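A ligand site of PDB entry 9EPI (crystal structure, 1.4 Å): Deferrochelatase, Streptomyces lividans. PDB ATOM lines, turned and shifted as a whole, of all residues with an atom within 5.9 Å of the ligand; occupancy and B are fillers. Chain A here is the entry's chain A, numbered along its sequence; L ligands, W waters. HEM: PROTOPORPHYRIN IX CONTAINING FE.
Merely in contact with the ligand: Pro 285, Lys 191, Phe 316, Phe 250, Phe 327, His 284, Gln 331, Asn 186, Ala 283, Asp 192, Leu 339, Val 280, Phe 190, Met 233, Leu 188, Arg 252, Ile 231, Leu 314, Val 330, Leu 334 and Ile 343.
26 residues have an atom within 4 Å of the ligand: Asn 186, Leu 188, Phe 190, Lys 191, Asp 192, Gly 193, Thr 194, Arg 195, Ile 231, Met 233, Phe 250, Arg 252, His 279, Val 280, Ala 283, His 284, Pro 285, Arg 295, Leu 314, Phe 316, Phe 327, Val 330, Gln 331, Leu 334, Leu 339 and Ile 343.
The nearest printed residue that does not touch the ligand is Leu 293 (4.002 Å).
The guanidinium group (NH2) of Arg 295 sits at hydrogen-bond distance from the backbone carbonyl oxygen (O) of Arg 195, 2.9 Å away.
NH1 of Arg 295 is in salt-bridge range of OD1 of Asp 192 (3.2 Å).
The side-chain amide oxygen (OD1) of Asn 196 sits at hydrogen-bond distance from the backbone NH (N) of Arg 295, 2.8 Å away.
The guanidinium group of Arg 195 is in hydrogen-bond range of a ring nitrogen (NE2) of His 284, at 3.3 Å.
The backbone NH of Phe 316 sits at hydrogen-bond distance from the backbone carbonyl oxygen of Arg 229, at 2.8 Å.
The backbone carbonyl oxygen (O) of Phe 250 lies within hydrogen-bond range of the backbone NH (N) of Val 280 (3.1 Å).
The side-chain amide nitrogen of Asn 186 sits close to the backbone carbonyl oxygen of Phe 190 (3.5 Å).
N of Leu 314 sits at hydrogen-bond distance from O of Ile 231 (2.9 Å).
Water W7 lies within hydrogen-bond range of the side-chain carboxylate (OD1) of Asp 192 (2.8 Å) and the guanidinium group (NH1) of Arg 295 (2.9 Å).
Water W6 lies within hydrogen-bond range of O1D of the ligand (2.7 Å) and NH2 of Arg 252 (2.8 Å).
Water W4 bridges an oxygen (O2D) of the ligand (2.7 Å) and the backbone carbonyl oxygen (O) of Arg 195 (2.8 Å).
Water W1 bridges NE2 of His 345 (2.8 Å) and OE1 of Gln 331 (3.0 Å).
NE2 of His 279 binds FE of the ligand (2.1 Å).
An oxygen (O1A) of the ligand lies within hydrogen-bond range of the backbone NH of Gly 193, at 2.7 Å.
NH1 of Arg 295 lies within salt-bridge range of O1A of the ligand (2.9 Å).
The backbone NH (N) of Arg 195 is in hydrogen-bond range of an oxygen (O2A) of the ligand, at 3.0 Å.
O1D of the ligand is in salt-bridge range of NE of Arg 195 (2.9 Å).
The backbone NH of Thr 194 sits at hydrogen-bond distance from an oxygen (O1A) of the ligand, 3.3 Å away.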
ATOM      1  N   ASN A 186      -7.344 -20.958 -16.574  1.00  0.00           N
ATOM      2  CA  ASN A 186      -7.059 -22.311 -16.081  1.00  0.00           C
ATOM      3  C   ASN A 186      -7.278 -22.350 -14.550  1.00  0.00           C
ATOM      4  O   ASN A 186      -7.620 -21.344 -13.937  1.00  0.00           O
ATOM      5  CB  ASN A 186      -5.666 -22.751 -16.482  1.00  0.00           C
ATOM      6  CG  ASN A 186      -4.615 -21.805 -15.999  1.00  0.00           C
ATOM      7  OD1 ASN A 186      -4.614 -21.402 -14.816  1.00  0.00           O
ATOM      8  ND2 ASN A 186      -3.695 -21.468 -16.902  1.00  0.00           N
ATOM      9  N   LEU A 188      -5.204 -22.561 -12.177  1.00  0.00           N
ATOM     10  CA  LEU A 188      -4.292 -21.739 -11.394  1.00  0.00           C
ATOM     11  C   LEU A 188      -4.758 -20.290 -11.364  1.00  0.00           C
ATOM     12  O   LEU A 188      -4.142 -19.471 -10.688  1.00  0.00           O
ATOM     13  CB  LEU A 188      -2.883 -21.821 -11.947  1.00  0.00           C
ATOM     14  CG  LEU A 188      -2.273 -23.209 -12.074  1.00  0.00           C
ATOM     15  CD1 LEU A 188      -0.829 -23.124 -12.546  1.00  0.00           C
ATOM     16  CD2 LEU A 188      -2.379 -23.981 -10.759  1.00  0.00           C
ATOM     17  N   PHE A 190      -5.065 -18.080 -13.944  1.00  0.00           N
ATOM     18  CA  PHE A 190      -4.533 -17.213 -14.978  1.00  0.00           C
ATOM     19  C   PHE A 190      -5.234 -17.445 -16.299  1.00  0.00           C
ATOM     20  O   PHE A 190      -5.557 -18.559 -16.658  1.00  0.00           O
ATOM     21  CB  PHE A 190      -3.042 -17.493 -15.145  1.00  0.00           C
ATOM     22  CG  PHE A 190      -2.180 -16.809 -14.121  1.00  0.00           C
ATOM     23  CD1 PHE A 190      -2.127 -17.250 -12.810  1.00  0.00           C
ATOM     24  CD2 PHE A 190      -1.463 -15.657 -14.454  1.00  0.00           C
ATOM     25  CE1 PHE A 190      -1.322 -16.603 -11.873  1.00  0.00           C
ATOM     26  CE2 PHE A 190      -0.722 -15.002 -13.501  1.00  0.00           C
ATOM     27  CZ  PHE A 190      -0.652 -15.446 -12.224  1.00  0.00           C
ATOM     28  N   LYS A 191      -5.383 -16.371 -17.067  1.00  0.00           N
ATOM     29  CA  LYS A 191      -5.845 -16.437 -18.420  1.00  0.00           C
ATOM     30  C   LYS A 191      -4.869 -17.277 -19.243  1.00  0.00           C
ATOM     31  O   LYS A 191      -3.658 -17.140 -19.091  1.00  0.00           O
ATOM     32  CB  LYS A 191      -5.912 -15.044 -19.053  1.00  0.00           C
ATOM     33  CG  LYS A 191      -6.962 -14.140 -18.460  1.00  0.00           C
ATOM     34  CD  LYS A 191      -6.887 -12.745 -19.126  1.00  0.00           C
ATOM     35  CE  LYS A 191      -7.965 -11.818 -18.648  1.00  0.00           C
ATOM     36  NZ  LYS A 191      -7.805 -10.448 -19.183  1.00  0.00           N
ATOM     37  N   ASP A 192      -5.397 -18.158 -20.079  1.00  0.00           N
ATOM     38  CA  ASP A 192      -4.606 -19.111 -20.831  1.00  0.00           C
ATOM     39  C   ASP A 192      -5.146 -19.130 -22.233  1.00  0.00           C
ATOM     40  O   ASP A 192      -6.295 -19.486 -22.437  1.00  0.00           O
ATOM     41  CB  ASP A 192      -4.702 -20.475 -20.164  1.00  0.00           C
ATOM     42  CG  ASP A 192      -3.564 -21.429 -20.425  1.00  0.00           C
ATOM     43  OD1 ASP A 192      -2.838 -21.260 -21.402  1.00  0.00           O
ATOM     44  OD2 ASP A 192      -3.458 -22.351 -19.619  1.00  0.00           O
ATOM     45  N   GLY A 193      -4.345 -18.616 -23.179  1.00  0.00           N
ATOM     46  CA  GLY A 193      -4.708 -18.553 -24.581  1.00  0.00           C
ATOM     47  C   GLY A 193      -4.495 -17.195 -25.202  1.00  0.00           C
ATOM     48  O   GLY A 193      -4.822 -17.074 -26.362  1.00  0.00           O
ATOM     49  N   THR A 194      -3.997 -16.193 -24.489  1.00  0.00           N
ATOM     50  CA  THR A 194      -3.837 -14.869 -25.052  1.00  0.00           C
ATOM     51  C   THR A 194      -3.035 -14.889 -26.358  1.00  0.00           C
ATOM     52  O   THR A 194      -3.477 -14.312 -27.341  1.00  0.00           O
ATOM     53  CB  THR A 194      -3.194 -13.966 -24.020  1.00  0.00           C
ATOM     54  OG1 THR A 194      -3.977 -13.975 -22.839  1.00  0.00           O
ATOM     55  CG2 THR A 194      -2.991 -12.555 -24.544  1.00  0.00           C
ATOM     56  N   ARG A 195      -1.834 -15.437 -26.314  1.00  0.00           N
ATOM     57  CA  ARG A 195      -0.952 -15.451 -27.462  1.00  0.00           C
ATOM     58  C   ARG A 195      -0.942 -16.845 -28.075  1.00  0.00           C
ATOM     59  O   ARG A 195      -0.032 -17.642 -27.845  1.00  0.00           O
ATOM     60  CB  ARG A 195       0.462 -14.953 -27.138  1.00  0.00           C
ATOM     61  CG  ARG A 195       0.557 -13.446 -27.148  1.00  0.00           C
ATOM     62  CD  ARG A 195       1.869 -12.832 -26.763  1.00  0.00           C
ATOM     63  NE  ARG A 195       2.971 -13.556 -27.394  1.00  0.00           N
ATOM     64  CZ  ARG A 195       3.224 -13.617 -28.683  1.00  0.00           C
ATOM     65  NH1 ARG A 195       3.946 -14.590 -29.144  1.00  0.00           N
ATOM     66  NH2 ARG A 195       2.732 -12.704 -29.512  1.00  0.00           N
ATOM     67  N   ASN A 196      -1.969 -17.121 -28.866  1.00  0.00           N
ATOM     68  CA  ASN A 196      -2.129 -18.386 -29.540  1.00  0.00           C
ATOM     69  C   ASN A 196      -2.081 -18.103 -31.041  1.00  0.00           C
ATOM     70  O   ASN A 196      -1.244 -17.300 -31.517  1.00  0.00           O
ATOM     71  CB  ASN A 196      -3.325 -19.114 -28.913  1.00  0.00           C
ATOM     72  CG  ASN A 196      -3.349 -20.586 -29.266  1.00  0.00           C
ATOM     73  OD1 ASN A 196      -2.333 -21.279 -29.324  1.00  0.00           O
ATOM     74  ND2 ASN A 196      -4.524 -21.108 -29.501  1.00  0.00           N
ATOM     75  N   ARG A 229      -0.893 -33.934 -23.614  1.00  0.00           N
ATOM     76  CA  ARG A 229      -0.239 -34.173 -22.333  1.00  0.00           C
ATOM     77  C   ARG A 229      -1.221 -33.990 -21.197  1.00  0.00           C
ATOM     78  O   ARG A 229      -1.859 -32.946 -21.074  1.00  0.00           O
ATOM     79  CB  ARG A 229       0.935 -33.219 -22.154  1.00  0.00           C
ATOM     80  CG  ARG A 229       2.000 -33.287 -23.220  1.00  0.00           C
ATOM     81  CD  ARG A 229       2.871 -34.535 -23.190  1.00  0.00           C
ATOM     82  NE  ARG A 229       3.838 -34.398 -22.096  1.00  0.00           N
ATOM     83  CZ  ARG A 229       4.938 -35.113 -21.964  1.00  0.00           C
ATOM     84  NH1 ARG A 229       5.197 -36.094 -22.818  1.00  0.00           N
ATOM     85  NH2 ARG A 229       5.802 -34.762 -21.000  1.00  0.00           N
ATOM     86  N   ILE A 231      -1.627 -33.194 -17.524  1.00  0.00           N
ATOM     87  CA  ILE A 231      -0.761 -32.506 -16.587  1.00  0.00           C
ATOM     88  C   ILE A 231      -1.489 -32.311 -15.266  1.00  0.00           C
ATOM     89  O   ILE A 231      -2.526 -31.648 -15.200  1.00  0.00           O
ATOM     90  CB  ILE A 231      -0.279 -31.157 -17.154  1.00  0.00           C
ATOM     91  CG1 ILE A 231       0.323 -31.308 -18.499  1.00  0.00           C
ATOM     92  CG2 ILE A 231       0.688 -30.463 -16.181  1.00  0.00           C
ATOM     93  CD1 ILE A 231       0.712 -29.989 -19.159  1.00  0.00           C
ATOM     94  N   MET A 233      -1.862 -30.696 -11.589  1.00  0.00           N
ATOM     95  CA  MET A 233      -1.483 -29.441 -10.960  1.00  0.00           C
ATOM     96  C   MET A 233      -1.423 -29.663  -9.460  1.00  0.00           C
ATOM     97  O   MET A 233      -2.316 -30.234  -8.881  1.00  0.00           O
ATOM     98  CB  MET A 233      -2.511 -28.349 -11.254  1.00  0.00           C
ATOM     99  CG  MET A 233      -2.476 -27.878 -12.668  1.00  0.00           C
ATOM    100  SD  MET A 233      -3.932 -26.829 -12.987  1.00  0.00           S
ATOM    101  CE  MET A 233      -3.422 -25.958 -14.476  1.00  0.00           C
ATOM    102  N   PHE A 250       4.705 -16.830 -14.162  1.00  0.00           N
ATOM    103  CA  PHE A 250       4.213 -16.678 -15.521  1.00  0.00           C
ATOM    104  C   PHE A 250       4.862 -15.537 -16.302  1.00  0.00           C
ATOM    105  O   PHE A 250       5.109 -15.693 -17.500  1.00  0.00           O
ATOM    106  CB  PHE A 250       2.688 -16.559 -15.536  1.00  0.00           C
ATOM    107  CG  PHE A 250       2.038 -17.899 -15.288  1.00  0.00           C
ATOM    108  CD1 PHE A 250       2.178 -18.895 -16.234  1.00  0.00           C
ATOM    109  CD2 PHE A 250       1.330 -18.158 -14.137  1.00  0.00           C
ATOM    110  CE1 PHE A 250       1.675 -20.143 -16.007  1.00  0.00           C
ATOM    111  CE2 PHE A 250       0.804 -19.435 -13.916  1.00  0.00           C
ATOM    112  CZ  PHE A 250       0.990 -20.404 -14.854  1.00  0.00           C
ATOM    113  N   ARG A 252       3.113 -12.615 -16.294  1.00  0.00           N
ATOM    114  CA  ARG A 252       1.923 -11.809 -16.517  1.00  0.00           C
ATOM    115  C   ARG A 252       1.243 -11.619 -15.179  1.00  0.00           C
ATOM    116  O   ARG A 252       1.439 -12.441 -14.291  1.00  0.00           O
ATOM    117  CB  ARG A 252       0.963 -12.507 -17.463  1.00  0.00           C
ATOM    118  CG  ARG A 252       1.439 -12.512 -18.891  1.00  0.00           C
ATOM    119  CD  ARG A 252       0.509 -13.259 -19.813  1.00  0.00           C
ATOM    120  NE  ARG A 252       0.869 -13.165 -21.230  1.00  0.00           N
ATOM    121  CZ  ARG A 252       0.507 -12.245 -22.095  1.00  0.00           C
ATOM    122  NH1 ARG A 252      -0.249 -11.205 -21.756  1.00  0.00           N
ATOM    123  NH2 ARG A 252       0.853 -12.412 -23.354  1.00  0.00           N
ATOM    124  N   PRO A 269       4.389  -8.865 -24.908  1.00  0.00           N
ATOM    125  CA  PRO A 269       5.374  -9.078 -23.875  1.00  0.00           C
ATOM    126  C   PRO A 269       6.702  -8.404 -24.165  1.00  0.00           C
ATOM    127  O   PRO A 269       7.125  -8.410 -25.302  1.00  0.00           O
ATOM    128  CB  PRO A 269       5.557 -10.585 -23.803  1.00  0.00           C
ATOM    129  CG  PRO A 269       4.577 -11.155 -24.742  1.00  0.00           C
ATOM    130  CD  PRO A 269       3.886 -10.073 -25.539  1.00  0.00           C
ATOM    131  N   HIS A 279       7.428 -18.712 -17.257  1.00  0.00           N
ATOM    132  CA  HIS A 279       6.833 -19.560 -18.277  1.00  0.00           C
ATOM    133  C   HIS A 279       6.715 -18.875 -19.627  1.00  0.00           C
ATOM    134  O   HIS A 279       7.039 -19.490 -20.635  1.00  0.00           O
ATOM    135  CB  HIS A 279       5.505 -20.102 -17.749  1.00  0.00           C
ATOM    136  CG  HIS A 279       4.798 -21.009 -18.672  1.00  0.00           C
ATOM    137  ND1 HIS A 279       5.170 -22.312 -18.894  1.00  0.00           N
ATOM    138  CD2 HIS A 279       3.697 -20.790 -19.458  1.00  0.00           C
ATOM    139  CE1 HIS A 279       4.340 -22.836 -19.809  1.00  0.00           C
ATOM    140  NE2 HIS A 279       3.405 -21.950 -20.138  1.00  0.00           N
ATOM    141  N   VAL A 280       6.147 -17.669 -19.651  1.00  0.00           N
ATOM    142  CA  VAL A 280       5.935 -16.971 -20.904  1.00  0.00           C
ATOM    143  C   VAL A 280       7.262 -16.700 -21.573  1.00  0.00           C
ATOM    144  O   VAL A 280       7.336 -16.822 -22.778  1.00  0.00           O
ATOM    145  CB  VAL A 280       5.100 -15.711 -20.721  1.00  0.00           C
ATOM    146  CG1 VAL A 280       5.071 -14.849 -21.971  1.00  0.00           C
ATOM    147  CG2 VAL A 280       3.682 -16.070 -20.300  1.00  0.00           C
ATOM    148  N   ALA A 283       8.519 -20.016 -23.097  1.00  0.00           N
ATOM    149  CA  ALA A 283       7.643 -20.610 -24.098  1.00  0.00           C
ATOM    150  C   ALA A 283       7.481 -19.759 -25.334  1.00  0.00           C
ATOM    151  O   ALA A 283       6.983 -20.274 -26.338  1.00  0.00           O
ATOM    152  CB  ALA A 283       6.263 -20.878 -23.483  1.00  0.00           C
ATOM    153  N   HIS A 284       7.810 -18.471 -25.267  1.00  0.00           N
ATOM    154  CA  HIS A 284       7.538 -17.524 -26.354  1.00  0.00           C
ATOM    155  C   HIS A 284       8.295 -17.934 -27.609  1.00  0.00           C
ATOM    156  O   HIS A 284       9.409 -18.415 -27.506  1.00  0.00           O
ATOM    157  CB  HIS A 284       8.001 -16.139 -25.910  1.00  0.00           C
ATOM    158  CG  HIS A 284       7.509 -15.031 -26.741  1.00  0.00           C
ATOM    159  ND1 HIS A 284       8.115 -14.685 -27.945  1.00  0.00           N
ATOM    160  CD2 HIS A 284       6.545 -14.114 -26.532  1.00  0.00           C
ATOM    161  CE1 HIS A 284       7.500 -13.640 -28.457  1.00  0.00           C
ATOM    162  NE2 HIS A 284       6.536 -13.257 -27.619  1.00  0.00           N
ATOM    163  N   PRO A 285       7.704 -17.783 -28.815  1.00  0.00           N
ATOM    164  CA  PRO A 285       8.380 -18.106 -30.061  1.00  0.00           C
ATOM    165  C   PRO A 285       9.770 -17.487 -30.176  1.00  0.00           C
ATOM    166  O   PRO A 285      10.662 -18.160 -30.693  1.00  0.00           O
ATOM    167  CB  PRO A 285       7.405 -17.571 -31.111  1.00  0.00           C
ATOM    168  CG  PRO A 285       6.073 -17.771 -30.467  1.00  0.00           C
ATOM    169  CD  PRO A 285       6.311 -17.347 -29.058  1.00  0.00           C
ATOM    170  N   LEU A 293       2.919 -22.723 -31.590  1.00  0.00           N
ATOM    171  CA  LEU A 293       1.994 -23.841 -31.460  1.00  0.00           C
ATOM    172  C   LEU A 293       0.578 -23.313 -31.487  1.00  0.00           C
ATOM    173  O   LEU A 293       0.330 -22.177 -31.119  1.00  0.00           O
ATOM    174  CB  LEU A 293       2.152 -24.457 -30.059  1.00  0.00           C
ATOM    175  CG  LEU A 293       3.515 -24.962 -29.636  1.00  0.00           C
ATOM    176  CD1 LEU A 293       3.486 -25.437 -28.195  1.00  0.00           C
ATOM    177  CD2 LEU A 293       3.874 -26.119 -30.545  1.00  0.00           C
ATOM    178  N   ARG A 295      -2.434 -24.056 -29.269  1.00  0.00           N
ATOM    179  CA  ARG A 295      -2.815 -24.681 -28.031  1.00  0.00           C
ATOM    180  C   ARG A 295      -4.313 -24.755 -27.948  1.00  0.00           C
ATOM    181  O   ARG A 295      -4.999 -23.782 -28.278  1.00  0.00           O
ATOM    182  CB  ARG A 295      -2.305 -23.871 -26.842  1.00  0.00           C
ATOM    183  CG  ARG A 295      -0.794 -23.898 -26.745  1.00  0.00           C
ATOM    184  CD  ARG A 295      -0.275 -23.061 -25.635  1.00  0.00           C
ATOM    185  NE  ARG A 295      -0.396 -21.660 -26.021  1.00  0.00           N
ATOM    186  CZ  ARG A 295      -0.784 -20.666 -25.267  1.00  0.00           C
ATOM    187  NH1 ARG A 295      -1.144 -20.864 -24.034  1.00  0.00           N
ATOM    188  NH2 ARG A 295      -0.858 -19.439 -25.761  1.00  0.00           N
ATOM    189  N   LEU A 314      -4.738 -30.105 -16.142  1.00  0.00           N
ATOM    190  CA  LEU A 314      -4.897 -29.501 -17.449  1.00  0.00           C
ATOM    191  C   LEU A 314      -4.560 -30.558 -18.478  1.00  0.00           C
ATOM    192  O   LEU A 314      -3.514 -31.183 -18.423  1.00  0.00           O
ATOM    193  CB  LEU A 314      -4.032 -28.242 -17.545  1.00  0.00           C
ATOM    194  CG  LEU A 314      -4.372 -27.277 -18.673  1.00  0.00           C
ATOM    195  CD1 LEU A 314      -4.025 -25.872 -18.309  1.00  0.00           C
ATOM    196  CD2 LEU A 314      -3.689 -27.667 -19.945  1.00  0.00           C
ATOM    197  N   PHE A 316      -3.501 -30.841 -21.871  1.00  0.00           N
ATOM    198  CA  PHE A 316      -2.846 -29.926 -22.786  1.00  0.00           C
ATOM    199  C   PHE A 316      -2.883 -30.530 -24.172  1.00  0.00           C
ATOM    200  O   PHE A 316      -2.490 -31.665 -24.339  1.00  0.00           O
ATOM    201  CB  PHE A 316      -1.396 -29.748 -22.310  1.00  0.00           C
ATOM    202  CG  PHE A 316      -0.630 -28.799 -23.196  1.00  0.00           C
ATOM    203  CD1 PHE A 316      -0.711 -27.431 -22.958  1.00  0.00           C
ATOM    204  CD2 PHE A 316       0.159 -29.252 -24.237  1.00  0.00           C
ATOM    205  CE1 PHE A 316       0.029 -26.535 -23.735  1.00  0.00           C
ATOM    206  CE2 PHE A 316       0.854 -28.352 -25.018  1.00  0.00           C
ATOM    207  CZ  PHE A 316       0.777 -27.006 -24.740  1.00  0.00           C
ATOM    208  N   PHE A 327       6.143 -28.709 -30.567  1.00  0.00           N
ATOM    209  CA  PHE A 327       6.117 -29.050 -29.159  1.00  0.00           C
ATOM    210  C   PHE A 327       7.512 -29.389 -28.618  1.00  0.00           C
ATOM    211  O   PHE A 327       7.843 -28.995 -27.511  1.00  0.00           O
ATOM    212  CB  PHE A 327       5.171 -30.221 -28.944  1.00  0.00           C
ATOM    213  CG  PHE A 327       5.079 -30.699 -27.503  1.00  0.00           C
ATOM    214  CD1 PHE A 327       4.280 -30.003 -26.609  1.00  0.00           C
ATOM    215  CD2 PHE A 327       5.893 -31.706 -27.009  1.00  0.00           C
ATOM    216  CE1 PHE A 327       4.225 -30.359 -25.277  1.00  0.00           C
ATOM    217  CE2 PHE A 327       5.800 -32.080 -25.679  1.00  0.00           C
ATOM    218  CZ  PHE A 327       4.992 -31.398 -24.799  1.00  0.00           C
ATOM    219  N   VAL A 330       9.833 -26.373 -27.669  1.00  0.00           N
ATOM    220  CA  VAL A 330       9.280 -25.541 -26.651  1.00  0.00           C
ATOM    221  C   VAL A 330       9.310 -26.298 -25.328  1.00  0.00           C
ATOM    222  O   VAL A 330       9.751 -25.740 -24.319  1.00  0.00           O
ATOM    223  CB  VAL A 330       7.886 -25.058 -27.048  1.00  0.00           C
ATOM    224  CG1 VAL A 330       7.254 -24.260 -25.936  1.00  0.00           C
ATOM    225  CG2 VAL A 330       7.946 -24.261 -28.334  1.00  0.00           C
ATOM    226  N   GLN A 331       8.886 -27.567 -25.290  1.00  0.00           N
ATOM    227  CA  GLN A 331       8.925 -28.292 -24.038  1.00  0.00           C
ATOM    228  C   GLN A 331      10.376 -28.465 -23.537  1.00  0.00           C
ATOM    229  O   GLN A 331      10.612 -28.417 -22.340  1.00  0.00           O
ATOM    230  CB  GLN A 331       8.175 -29.642 -24.178  1.00  0.00           C
ATOM    231  CG  GLN A 331       8.133 -30.521 -22.944  1.00  0.00           C
ATOM    232  CD  GLN A 331       7.445 -29.899 -21.748  1.00  0.00           C
ATOM    233  OE1 GLN A 331       6.483 -29.151 -21.885  1.00  0.00           O
ATOM    234  NE2 GLN A 331       7.918 -30.223 -20.562  1.00  0.00           N
ATOM    235  N   LEU A 334      11.324 -25.610 -21.572  1.00  0.00           N
ATOM    236  CA  LEU A 334      10.640 -25.476 -20.292  1.00  0.00           C
ATOM    237  C   LEU A 334      11.312 -26.307 -19.207  1.00  0.00           C
ATOM    238  O   LEU A 334      10.785 -26.417 -18.091  1.00  0.00           O
ATOM    239  CB  LEU A 334       9.161 -25.843 -20.392  1.00  0.00           C
ATOM    240  CG  LEU A 334       8.360 -24.982 -21.370  1.00  0.00           C
ATOM    241  CD1 LEU A 334       6.855 -25.369 -21.299  1.00  0.00           C
ATOM    242  CD2 LEU A 334       8.487 -23.537 -21.140  1.00  0.00           C
ATOM    243  N   LEU A 339       7.239 -22.891 -13.482  1.00  0.00           N
ATOM    244  CA  LEU A 339       5.980 -23.595 -13.387  1.00  0.00           C
ATOM    245  C   LEU A 339       6.171 -25.061 -13.026  1.00  0.00           C
ATOM    246  O   LEU A 339       5.275 -25.691 -12.455  1.00  0.00           O
ATOM    247  CB  LEU A 339       5.221 -23.478 -14.697  1.00  0.00           C
ATOM    248  CG  LEU A 339       3.805 -24.050 -14.701  1.00  0.00           C
ATOM    249  CD1 LEU A 339       2.888 -23.438 -13.667  1.00  0.00           C
ATOM    250  CD2 LEU A 339       3.220 -23.925 -16.095  1.00  0.00           C
ATOM    251  N   ILE A 343       3.515 -28.562 -11.309  1.00  0.00           N
ATOM    252  CA  ILE A 343       2.854 -29.433 -12.267  1.00  0.00           C
ATOM    253  C   ILE A 343       3.643 -30.722 -12.406  1.00  0.00           C
ATOM    254  O   ILE A 343       4.798 -30.781 -12.035  1.00  0.00           O
ATOM    255  CB  ILE A 343       2.696 -28.770 -13.639  1.00  0.00           C
ATOM    256  CG1 ILE A 343       4.039 -28.512 -14.298  1.00  0.00           C
ATOM    257  CG2 ILE A 343       1.850 -27.520 -13.535  1.00  0.00           C
ATOM    258  CD1 ILE A 343       3.926 -28.181 -15.778  1.00  0.00           C
ATOM    259  N   HIS A 345       3.702 -33.854 -15.599  1.00  0.00           N
ATOM    260  CA  HIS A 345       3.115 -34.532 -16.738  1.00  0.00           C
ATOM    261  C   HIS A 345       2.943 -36.003 -16.390  1.00  0.00           C
ATOM    262  O   HIS A 345       3.934 -36.663 -16.057  1.00  0.00           O
ATOM    263  CB  HIS A 345       3.986 -34.349 -17.951  1.00  0.00           C
ATOM    264  CG  HIS A 345       4.116 -32.947 -18.423  1.00  0.00           C
ATOM    265  ND1 HIS A 345       3.883 -32.653 -19.749  1.00  0.00           N
ATOM    266  CD2 HIS A 345       4.499 -31.825 -17.835  1.00  0.00           C
ATOM    267  CE1 HIS A 345       4.088 -31.350 -19.930  1.00  0.00           C
ATOM    268  NE2 HIS A 345       4.514 -30.832 -18.784  1.00  0.00           N
HETATM  269  CHA HEM L   1       1.410 -19.205 -22.360  1.00  0.00           C
HETATM  270  CHB HEM L   1      -0.198 -21.509 -18.454  1.00  0.00           C
HETATM  271  CHC HEM L   1       1.704 -25.636 -20.055  1.00  0.00           C
HETATM  272  CHD HEM L   1       3.173 -23.324 -24.009  1.00  0.00           C
HETATM  273  C1A HEM L   1       0.833 -19.433 -21.140  1.00  0.00           C
HETATM  274  C2A HEM L   1       0.170 -18.459 -20.348  1.00  0.00           C
HETATM  275  C3A HEM L   1      -0.278 -19.103 -19.222  1.00  0.00           C
HETATM  276  C4A HEM L   1       0.096 -20.466 -19.365  1.00  0.00           C
HETATM  277  CMA HEM L   1      -1.009 -18.515 -18.029  1.00  0.00           C
HETATM  278  CAA HEM L   1       0.061 -16.986 -20.660  1.00  0.00           C
HETATM  279  CBA HEM L   1      -1.128 -16.580 -21.532  1.00  0.00           C
HETATM  280  CGA HEM L   1      -1.071 -17.101 -22.899  1.00  0.00           C
HETATM  281  O1A HEM L   1      -1.656 -18.172 -23.213  1.00  0.00           O
HETATM  282  O2A HEM L   1      -0.456 -16.484 -23.803  1.00  0.00           O
HETATM  283  C1B HEM L   1       0.150 -22.845 -18.580  1.00  0.00           C
HETATM  284  C2B HEM L   1      -0.189 -23.836 -17.586  1.00  0.00           C
HETATM  285  C3B HEM L   1       0.359 -24.988 -18.040  1.00  0.00           C
HETATM  286  C4B HEM L   1       1.050 -24.705 -19.293  1.00  0.00           C
HETATM  287  CMB HEM L   1      -0.969 -23.603 -16.307  1.00  0.00           C
HETATM  288  CAB HEM L   1       0.319 -26.374 -17.513  1.00  0.00           C
HETATM  289  CBB HEM L   1      -0.520 -26.811 -16.635  1.00  0.00           C
HETATM  290  C1C HEM L   1       2.313 -25.400 -21.267  1.00  0.00           C
HETATM  291  C2C HEM L   1       3.024 -26.330 -22.064  1.00  0.00           C
HETATM  292  C3C HEM L   1       3.440 -25.687 -23.190  1.00  0.00           C
HETATM  293  C4C HEM L   1       3.024 -24.309 -23.072  1.00  0.00           C
HETATM  294  CMC HEM L   1       3.155 -27.745 -21.705  1.00  0.00           C
HETATM  295  CAC HEM L   1       4.237 -26.154 -24.330  1.00  0.00           C
HETATM  296  CBC HEM L   1       4.989 -27.170 -24.358  1.00  0.00           C
HETATM  297  C1D HEM L   1       2.735 -22.012 -23.894  1.00  0.00           C
HETATM  298  C2D HEM L   1       2.962 -21.010 -24.950  1.00  0.00           C
HETATM  299  C3D HEM L   1       2.524 -19.834 -24.496  1.00  0.00           C
HETATM  300  C4D HEM L   1       1.988 -20.146 -23.143  1.00  0.00           C
HETATM  301  CMD HEM L   1       3.597 -21.300 -26.306  1.00  0.00           C
HETATM  302  CAD HEM L   1       2.464 -18.521 -25.171  1.00  0.00           C
HETATM  303  CBD HEM L   1       3.789 -17.740 -25.000  1.00  0.00           C
HETATM  304  CGD HEM L   1       3.802 -16.514 -25.842  1.00  0.00           C
HETATM  305  O1D HEM L   1       3.578 -15.411 -25.280  1.00  0.00           O
HETATM  306  O2D HEM L   1       3.968 -16.641 -27.077  1.00  0.00           O
HETATM  307  NA  HEM L   1       0.763 -20.675 -20.520  1.00  0.00           N
HETATM  308  NB  HEM L   1       0.857 -23.397 -19.543  1.00  0.00           N
HETATM  309  NC  HEM L   1       2.311 -24.182 -21.910  1.00  0.00           N
HETATM  310  ND  HEM L   1       2.146 -21.444 -22.839  1.00  0.00           N
HETATM  311 FE   HEM L   1       1.624 -22.367 -21.157  1.00  0.00          FE
HETATM  312  O   HOH W   1       5.485 -28.249 -19.153  1.00  0.00           O
HETATM  313  O   HOH W   2      -2.110 -24.491 -20.605  1.00  0.00           O
HETATM  314  O   HOH W   3       3.252 -20.579 -29.582  1.00  0.00           O
HETATM  315  O   HOH W   4       2.483 -17.965 -28.963  1.00  0.00           O
HETATM  316  O   HOH W   5       5.884 -21.146 -28.755  1.00  0.00           O
HETATM  317  O   HOH W   6       1.815 -15.092 -23.273  1.00  0.00           O
HETATM  318  O   HOH W   7      -0.546 -22.775 -21.954  1.00  0.00           O
